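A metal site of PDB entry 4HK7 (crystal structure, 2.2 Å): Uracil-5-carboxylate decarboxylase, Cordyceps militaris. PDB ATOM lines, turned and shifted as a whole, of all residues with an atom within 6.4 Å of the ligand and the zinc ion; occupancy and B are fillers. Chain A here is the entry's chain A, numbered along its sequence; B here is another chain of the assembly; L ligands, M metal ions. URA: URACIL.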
ATOM      1  N   HIS A  15     -22.529  17.680  10.361  1.00  0.00           N
ATOM      2  CA  HIS A  15     -22.277  17.305   8.970  1.00  0.00           C
ATOM      3  C   HIS A  15     -22.118  15.821   8.895  1.00  0.00           C
ATOM      4  O   HIS A  15     -21.015  15.299   9.027  1.00  0.00           O
ATOM      5  CB  HIS A  15     -21.050  18.035   8.420  1.00  0.00           C
ATOM      6  CG  HIS A  15     -20.882  17.874   6.926  1.00  0.00           C
ATOM      7  ND1 HIS A  15     -20.281  18.813   6.166  1.00  0.00           N
ATOM      8  CD2 HIS A  15     -21.283  16.861   6.059  1.00  0.00           C
ATOM      9  CE1 HIS A  15     -20.277  18.402   4.883  1.00  0.00           C
ATOM     10  NE2 HIS A  15     -20.891  17.213   4.819  1.00  0.00           N
ATOM     11  N   THR A  16     -23.222  15.131   8.653  1.00  0.00           N
ATOM     12  CA  THR A  16     -23.286  13.674   8.798  1.00  0.00           C
ATOM     13  C   THR A  16     -24.545  13.181   8.095  1.00  0.00           C
ATOM     14  O   THR A  16     -25.627  13.791   8.221  1.00  0.00           O
ATOM     15  CB  THR A  16     -23.223  13.256  10.296  1.00  0.00           C
ATOM     16  OG1 THR A  16     -23.491  11.860  10.443  1.00  0.00           O
ATOM     17  CG2 THR A  16     -24.204  14.054  11.154  1.00  0.00           C
ATOM     18  N   HIS A  17     -24.419  12.098   7.330  1.00  0.00           N
ATOM     19  CA  HIS A  17     -25.468  11.700   6.387  1.00  0.00           C
ATOM     20  C   HIS A  17     -25.990  10.296   6.511  1.00  0.00           C
ATOM     21  O   HIS A  17     -25.370   9.416   7.122  1.00  0.00           O
ATOM     22  CB  HIS A  17     -24.968  11.847   4.959  1.00  0.00           C
ATOM     23  CG  HIS A  17     -24.389  13.209   4.647  1.00  0.00           C
ATOM     24  ND1 HIS A  17     -25.158  14.300   4.494  1.00  0.00           N
ATOM     25  CD2 HIS A  17     -23.078  13.602   4.424  1.00  0.00           C
ATOM     26  CE1 HIS A  17     -24.365  15.351   4.204  1.00  0.00           C
ATOM     27  NE2 HIS A  17     -23.106  14.922   4.151  1.00  0.00           N
ATOM     28  N   TYR A  19     -28.567   7.508   3.783  1.00  0.00           N
ATOM     29  CA  TYR A  19     -29.548   7.210   2.738  1.00  0.00           C
ATOM     30  C   TYR A  19     -30.583   6.233   3.308  1.00  0.00           C
ATOM     31  O   TYR A  19     -30.264   5.057   3.510  1.00  0.00           O
ATOM     32  CB  TYR A  19     -28.892   6.542   1.528  1.00  0.00           C
ATOM     33  CG  TYR A  19     -27.932   7.391   0.730  1.00  0.00           C
ATOM     34  CD1 TYR A  19     -28.302   8.637   0.241  1.00  0.00           C
ATOM     35  CD2 TYR A  19     -26.665   6.911   0.408  1.00  0.00           C
ATOM     36  CE1 TYR A  19     -27.436   9.399  -0.519  1.00  0.00           C
ATOM     37  CE2 TYR A  19     -25.772   7.663  -0.352  1.00  0.00           C
ATOM     38  CZ  TYR A  19     -26.172   8.909  -0.808  1.00  0.00           C
ATOM     39  OH  TYR A  19     -25.313   9.675  -1.556  1.00  0.00           O
ATOM     40  N   LEU A  49     -22.409   8.222  -7.690  1.00  0.00           N
ATOM     41  CA  LEU A  49     -23.120   9.491  -7.482  1.00  0.00           C
ATOM     42  C   LEU A  49     -22.665  10.624  -8.389  1.00  0.00           C
ATOM     43  O   LEU A  49     -23.462  11.509  -8.727  1.00  0.00           O
ATOM     44  CB  LEU A  49     -22.951   9.953  -6.033  1.00  0.00           C
ATOM     45  CG  LEU A  49     -23.376   9.010  -4.905  1.00  0.00           C
ATOM     46  CD1 LEU A  49     -22.827   9.536  -3.584  1.00  0.00           C
ATOM     47  CD2 LEU A  49     -24.895   8.869  -4.865  1.00  0.00           C
ATOM     48  N   LEU A  50     -21.383  10.614  -8.758  1.00  0.00           N
ATOM     49  CA  LEU A  50     -20.732  11.776  -9.351  1.00  0.00           C
ATOM     50  C   LEU A  50     -20.452  11.609 -10.834  1.00  0.00           C
ATOM     51  O   LEU A  50     -20.181  10.501 -11.308  1.00  0.00           O
ATOM     52  CB  LEU A  50     -19.427  12.073  -8.611  1.00  0.00           C
ATOM     53  CG  LEU A  50     -19.437  12.032  -7.069  1.00  0.00           C
ATOM     54  CD1 LEU A  50     -18.012  11.941  -6.515  1.00  0.00           C
ATOM     55  CD2 LEU A  50     -20.202  13.195  -6.456  1.00  0.00           C
ATOM     56  N   ARG A  71     -18.030   4.245  -5.246  1.00  0.00           N
ATOM     57  CA  ARG A  71     -17.581   3.870  -3.899  1.00  0.00           C
ATOM     58  C   ARG A  71     -18.446   2.741  -3.319  1.00  0.00           C
ATOM     59  O   ARG A  71     -19.575   2.541  -3.788  1.00  0.00           O
ATOM     60  CB  ARG A  71     -17.569   5.091  -2.981  1.00  0.00           C
ATOM     61  CG  ARG A  71     -16.444   6.061  -3.284  1.00  0.00           C
ATOM     62  CD  ARG A  71     -16.692   7.422  -2.655  1.00  0.00           C
ATOM     63  NE  ARG A  71     -17.849   8.108  -3.229  1.00  0.00           N
ATOM     64  CZ  ARG A  71     -18.213   9.352  -2.925  1.00  0.00           C
ATOM     65  NH1 ARG A  71     -17.508  10.055  -2.038  1.00  0.00           N
ATOM     66  NH2 ARG A  71     -19.280   9.898  -3.501  1.00  0.00           N
ATOM     67  N   ALA A 100     -27.792  12.609   1.986  1.00  0.00           N
ATOM     68  CA  ALA A 100     -26.576  12.964   1.252  1.00  0.00           C
ATOM     69  C   ALA A 100     -26.927  13.342  -0.175  1.00  0.00           C
ATOM     70  O   ALA A 100     -28.008  13.029  -0.666  1.00  0.00           O
ATOM     71  CB  ALA A 100     -25.573  11.814   1.279  1.00  0.00           C
ATOM     72  N   ASN A 101     -25.998  14.028  -0.836  1.00  0.00           N
ATOM     73  CA  ASN A 101     -26.096  14.314  -2.256  1.00  0.00           C
ATOM     74  C   ASN A 101     -26.350  13.012  -3.036  1.00  0.00           C
ATOM     75  O   ASN A 101     -25.831  11.958  -2.662  1.00  0.00           O
ATOM     76  CB  ASN A 101     -24.802  14.983  -2.733  1.00  0.00           C
ATOM     77  CG  ASN A 101     -23.556  14.179  -2.378  1.00  0.00           C
ATOM     78  OD1 ASN A 101     -23.222  14.015  -1.199  1.00  0.00           O
ATOM     79  ND2 ASN A 101     -22.859  13.689  -3.398  1.00  0.00           N
ATOM     80  N   PHE A 196     -28.418  24.467   5.221  1.00  0.00           N
ATOM     81  CA  PHE A 196     -27.135  23.809   5.097  1.00  0.00           C
ATOM     82  C   PHE A 196     -26.846  23.646   3.609  1.00  0.00           C
ATOM     83  O   PHE A 196     -27.490  22.864   2.911  1.00  0.00           O
ATOM     84  CB  PHE A 196     -27.168  22.477   5.862  1.00  0.00           C
ATOM     85  CG  PHE A 196     -25.889  21.687   5.807  1.00  0.00           C
ATOM     86  CD1 PHE A 196     -24.651  22.318   5.701  1.00  0.00           C
ATOM     87  CD2 PHE A 196     -25.930  20.312   5.887  1.00  0.00           C
ATOM     88  CE1 PHE A 196     -23.476  21.576   5.655  1.00  0.00           C
ATOM     89  CE2 PHE A 196     -24.761  19.553   5.842  1.00  0.00           C
ATOM     90  CZ  PHE A 196     -23.534  20.194   5.720  1.00  0.00           C
ATOM     91  N   HIS A 198     -24.573  22.514   0.546  1.00  0.00           N
ATOM     92  CA  HIS A 198     -23.718  21.339   0.381  1.00  0.00           C
ATOM     93  C   HIS A 198     -23.448  21.072  -1.091  1.00  0.00           C
ATOM     94  O   HIS A 198     -24.361  21.140  -1.912  1.00  0.00           O
ATOM     95  CB  HIS A 198     -24.400  20.136   1.025  1.00  0.00           C
ATOM     96  CG  HIS A 198     -23.515  18.916   1.122  1.00  0.00           C
ATOM     97  ND1 HIS A 198     -23.226  18.161   0.053  1.00  0.00           N
ATOM     98  CD2 HIS A 198     -22.865  18.341   2.213  1.00  0.00           C
ATOM     99  CE1 HIS A 198     -22.423  17.133   0.428  1.00  0.00           C
ATOM    100  NE2 HIS A 198     -22.199  17.253   1.752  1.00  0.00           N
ATOM    101  N   PRO A 199     -22.179  20.752  -1.426  1.00  0.00           N
ATOM    102  CA  PRO A 199     -21.825  20.541  -2.836  1.00  0.00           C
ATOM    103  C   PRO A 199     -22.284  19.174  -3.372  1.00  0.00           C
ATOM    104  O   PRO A 199     -22.749  18.331  -2.605  1.00  0.00           O
ATOM    105  CB  PRO A 199     -20.295  20.575  -2.803  1.00  0.00           C
ATOM    106  CG  PRO A 199     -19.977  19.977  -1.463  1.00  0.00           C
ATOM    107  CD  PRO A 199     -21.022  20.567  -0.541  1.00  0.00           C
ATOM    108  N   HIS A 200     -22.156  18.986  -4.685  1.00  0.00           N
ATOM    109  CA  HIS A 200     -22.412  17.697  -5.346  1.00  0.00           C
ATOM    110  C   HIS A 200     -21.954  17.656  -6.768  1.00  0.00           C
ATOM    111  O   HIS A 200     -21.366  16.660  -7.210  1.00  0.00           O
ATOM    112  CB  HIS A 200     -23.901  17.339  -5.337  1.00  0.00           C
ATOM    113  CG  HIS A 200     -24.230  16.179  -6.246  1.00  0.00           C
ATOM    114  ND1 HIS A 200     -23.864  14.908  -5.965  1.00  0.00           N
ATOM    115  CD2 HIS A 200     -24.864  16.135  -7.482  1.00  0.00           C
ATOM    116  CE1 HIS A 200     -24.273  14.092  -6.956  1.00  0.00           C
ATOM    117  NE2 HIS A 200     -24.875  14.847  -7.887  1.00  0.00           N
ATOM    118  N   LEU A 221     -13.247  15.330  -5.072  1.00  0.00           N
ATOM    119  CA  LEU A 221     -13.642  15.475  -3.667  1.00  0.00           C
ATOM    120  C   LEU A 221     -12.854  16.532  -2.903  1.00  0.00           C
ATOM    121  O   LEU A 221     -13.423  17.274  -2.097  1.00  0.00           O
ATOM    122  CB  LEU A 221     -13.562  14.142  -2.908  1.00  0.00           C
ATOM    123  CG  LEU A 221     -14.505  13.011  -3.311  1.00  0.00           C
ATOM    124  CD1 LEU A 221     -14.230  11.785  -2.445  1.00  0.00           C
ATOM    125  CD2 LEU A 221     -15.972  13.429  -3.217  1.00  0.00           C
ATOM    126  N   PHE A 225     -15.648  19.772  -4.973  1.00  0.00           N
ATOM    127  CA  PHE A 225     -16.680  20.044  -3.968  1.00  0.00           C
ATOM    128  C   PHE A 225     -16.570  21.446  -3.319  1.00  0.00           C
ATOM    129  O   PHE A 225     -17.488  22.250  -3.440  1.00  0.00           O
ATOM    130  CB  PHE A 225     -16.675  18.938  -2.896  1.00  0.00           C
ATOM    131  CG  PHE A 225     -17.576  17.776  -3.188  1.00  0.00           C
ATOM    132  CD1 PHE A 225     -18.003  17.488  -4.486  1.00  0.00           C
ATOM    133  CD2 PHE A 225     -18.016  16.953  -2.153  1.00  0.00           C
ATOM    134  CE1 PHE A 225     -18.845  16.417  -4.746  1.00  0.00           C
ATOM    135  CE2 PHE A 225     -18.866  15.884  -2.400  1.00  0.00           C
ATOM    136  CZ  PHE A 225     -19.277  15.615  -3.703  1.00  0.00           C
ATOM    137  N   ALA A 253     -20.948  23.921   4.031  1.00  0.00           N
ATOM    138  CA  ALA A 253     -20.149  22.715   4.105  1.00  0.00           C
ATOM    139  C   ALA A 253     -18.679  23.009   3.858  1.00  0.00           C
ATOM    140  O   ALA A 253     -18.333  23.898   3.067  1.00  0.00           O
ATOM    141  CB  ALA A 253     -20.655  21.688   3.089  1.00  0.00           C
ATOM    142  N   HIS A 254     -17.824  22.265   4.558  1.00  0.00           N
ATOM    143  CA  HIS A 254     -16.371  22.300   4.347  1.00  0.00           C
ATOM    144  C   HIS A 254     -15.794  23.665   4.562  1.00  0.00           C
ATOM    145  O   HIS A 254     -15.026  24.177   3.730  1.00  0.00           O
ATOM    146  CB  HIS A 254     -16.037  21.727   2.973  1.00  0.00           C
ATOM    147  CG  HIS A 254     -16.748  20.429   2.673  1.00  0.00           C
ATOM    148  ND1 HIS A 254     -17.446  20.216   1.550  1.00  0.00           N
ATOM    149  CD2 HIS A 254     -16.867  19.266   3.443  1.00  0.00           C
ATOM    150  CE1 HIS A 254     -17.971  18.983   1.566  1.00  0.00           C
ATOM    151  NE2 HIS A 254     -17.618  18.402   2.733  1.00  0.00           N
ATOM    152  N   ASP A 326     -18.686  14.457   8.209  1.00  0.00           N
ATOM    153  CA  ASP A 326     -19.033  13.945   6.884  1.00  0.00           C
ATOM    154  C   ASP A 326     -19.208  12.419   6.858  1.00  0.00           C
ATOM    155  O   ASP A 326     -19.046  11.783   5.816  1.00  0.00           O
ATOM    156  CB  ASP A 326     -18.026  14.392   5.816  1.00  0.00           C
ATOM    157  CG  ASP A 326     -18.695  14.787   4.506  1.00  0.00           C
ATOM    158  OD1 ASP A 326     -19.886  14.460   4.320  1.00  0.00           O
ATOM    159  OD2 ASP A 326     -18.028  15.450   3.683  1.00  0.00           O
ATOM    160  N   HIS A 327     -19.545  11.839   8.018  1.00  0.00           N
ATOM    161  CA  HIS A 327     -19.881  10.405   8.098  1.00  0.00           C
ATOM    162  C   HIS A 327     -21.031  10.139   7.154  1.00  0.00           C
ATOM    163  O   HIS A 327     -21.946  10.950   7.090  1.00  0.00           O
ATOM    164  CB  HIS A 327     -20.253  10.041   9.531  1.00  0.00           C
ATOM    165  CG  HIS A 327     -20.542   8.569   9.726  1.00  0.00           C
ATOM    166  ND1 HIS A 327     -21.803   8.094   9.815  1.00  0.00           N
ATOM    167  CD2 HIS A 327     -19.698   7.477   9.844  1.00  0.00           C
ATOM    168  CE1 HIS A 327     -21.761   6.752   9.987  1.00  0.00           C
ATOM    169  NE2 HIS A 327     -20.477   6.385   9.996  1.00  0.00           N
ATOM    170  N   PHE A 329     -18.802   9.058   4.633  1.00  0.00           N
ATOM    171  CA  PHE A 329     -18.155   9.072   3.321  1.00  0.00           C
ATOM    172  C   PHE A 329     -16.648   8.753   3.320  1.00  0.00           C
ATOM    173  O   PHE A 329     -16.133   8.304   2.310  1.00  0.00           O
ATOM    174  CB  PHE A 329     -18.447  10.370   2.559  1.00  0.00           C
ATOM    175  CG  PHE A 329     -19.801  10.392   1.896  1.00  0.00           C
ATOM    176  CD1 PHE A 329     -19.996   9.781   0.648  1.00  0.00           C
ATOM    177  CD2 PHE A 329     -20.878  11.026   2.507  1.00  0.00           C
ATOM    178  CE1 PHE A 329     -21.239   9.817   0.031  1.00  0.00           C
ATOM    179  CE2 PHE A 329     -22.129  11.059   1.894  1.00  0.00           C
ATOM    180  CZ  PHE A 329     -22.308  10.448   0.654  1.00  0.00           C
ATOM    181  N   PHE A 330     -15.961   8.995   4.438  1.00  0.00           N
ATOM    182  CA  PHE A 330     -14.531   8.672   4.488  1.00  0.00           C
ATOM    183  C   PHE A 330     -14.169   7.645   5.579  1.00  0.00           C
ATOM    184  O   PHE A 330     -13.567   8.002   6.602  1.00  0.00           O
ATOM    185  CB  PHE A 330     -13.700   9.948   4.644  1.00  0.00           C
ATOM    186  CG  PHE A 330     -13.965  10.989   3.592  1.00  0.00           C
ATOM    187  CD1 PHE A 330     -13.300  10.950   2.374  1.00  0.00           C
ATOM    188  CD2 PHE A 330     -14.877  12.015   3.828  1.00  0.00           C
ATOM    189  CE1 PHE A 330     -13.549  11.913   1.397  1.00  0.00           C
ATOM    190  CE2 PHE A 330     -15.123  12.984   2.859  1.00  0.00           C
ATOM    191  CZ  PHE A 330     -14.449  12.929   1.650  1.00  0.00           C
ATOM    192  N   ARG B 265      -7.554  19.063   3.462  1.00  0.00           N
ATOM    193  CA  ARG B 265      -8.563  18.298   2.743  1.00  0.00           C
ATOM    194  C   ARG B 265      -7.951  17.356   1.689  1.00  0.00           C
ATOM    195  O   ARG B 265      -8.386  16.199   1.538  1.00  0.00           O
ATOM    196  CB  ARG B 265      -9.603  19.227   2.090  1.00  0.00           C
ATOM    197  CG  ARG B 265     -10.815  18.481   1.554  1.00  0.00           C
ATOM    198  CD  ARG B 265     -11.783  19.365   0.786  1.00  0.00           C
ATOM    199  NE  ARG B 265     -12.878  18.549   0.278  1.00  0.00           N
ATOM    200  CZ  ARG B 265     -13.837  18.016   1.042  1.00  0.00           C
ATOM    201  NH1 ARG B 265     -13.859  18.243   2.359  1.00  0.00           N
ATOM    202  NH2 ARG B 265     -14.781  17.258   0.501  1.00  0.00           N
HETATM  203  N1  URA L   1     -18.490  12.370  -1.073  1.00  0.00           N
HETATM  204  C2  URA L   1     -19.833  12.629  -1.429  1.00  0.00           C
HETATM  205  O2  URA L   1     -20.284  12.254  -2.507  1.00  0.00           O
HETATM  206  N3  URA L   1     -20.648  13.345  -0.548  1.00  0.00           N
HETATM  207  C4  URA L   1     -20.121  13.777   0.669  1.00  0.00           C
HETATM  208  O4  URA L   1     -20.846  14.393   1.457  1.00  0.00           O
HETATM  209  C5  URA L   1     -18.786  13.495   0.994  1.00  0.00           C
HETATM  210  C6  URA L   1     -17.994  12.781   0.093  1.00  0.00           C
HETATM  211 ZN    ZN M   1     -21.190  15.794   3.141  1.00  0.00          ZN
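The guanidinium group (NH2) of Arg 71 lies within hydrogen-bond range of an oxygen (O2) of the ligand (2.7 Å). The side-chain amide oxygen of Asn 101 sits at hydrogen-bond distance from a nitrogen (N3) of the ligand, at 2.7 Å.
The side-chain carboxylate (OD2) of Asp 326 is in hydrogen-bond range of a ring nitrogen (NE2) of His 254 (3.1 Å). The backbone NH of His 17 lies within hydrogen-bond range of the backbone carbonyl oxygen of His 327, 2.7 Å away. A ring nitrogen (ND1) of His 200 is in hydrogen-bond range of the side-chain amide nitrogen (ND2) of Asn 101 (3.0 Å). The backbone carbonyl oxygen of Asn 101 lies within hydrogen-bond range of the side-chain hydroxyl of Tyr 19 (2.6 Å). NE of Arg 265 of chain B sits at hydrogen-bond distance from O of Leu 221 (2.8 Å).
CD1 of Leu 49 touches O2 of the ligand (3.9 Å). Leu 221 touches the ligand (CD2 to N1, 3.5 Å). Phe 225 touches the ligand. CG of Phe 329 touches C5 of the ligand, 3.4 Å away. Phe 330 touches the ligand. Hydrophobic or aromatic side chains within 4 Å of the ligand: His 17, Leu 49, His 198, Leu 221, Phe 225, Phe 329 and Phe 330. Ten residues have an atom within 4 Å of the ligand: His 17, Leu 49, Arg 71, Asn 101, His 198, Leu 221, Phe 225, Asp 326, Phe 329 and Phe 330.
Along chain A the residues within 4 Å of the zinc ion span positions 15 to 326.
The zinc ion is bound by the side-chain carboxylate (OD1) of Asp 326 (2.2 Å), a ring nitrogen (NE2) of His 15 (2.2 Å), an oxygen (O4) of the ligand (2.2 Å), a ring nitrogen (NE2) of His 198 (2.3 Å) and a ring nitrogen (NE2) of His 17 (2.3 Å). The zinc ion has five donor atoms within binding distance.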
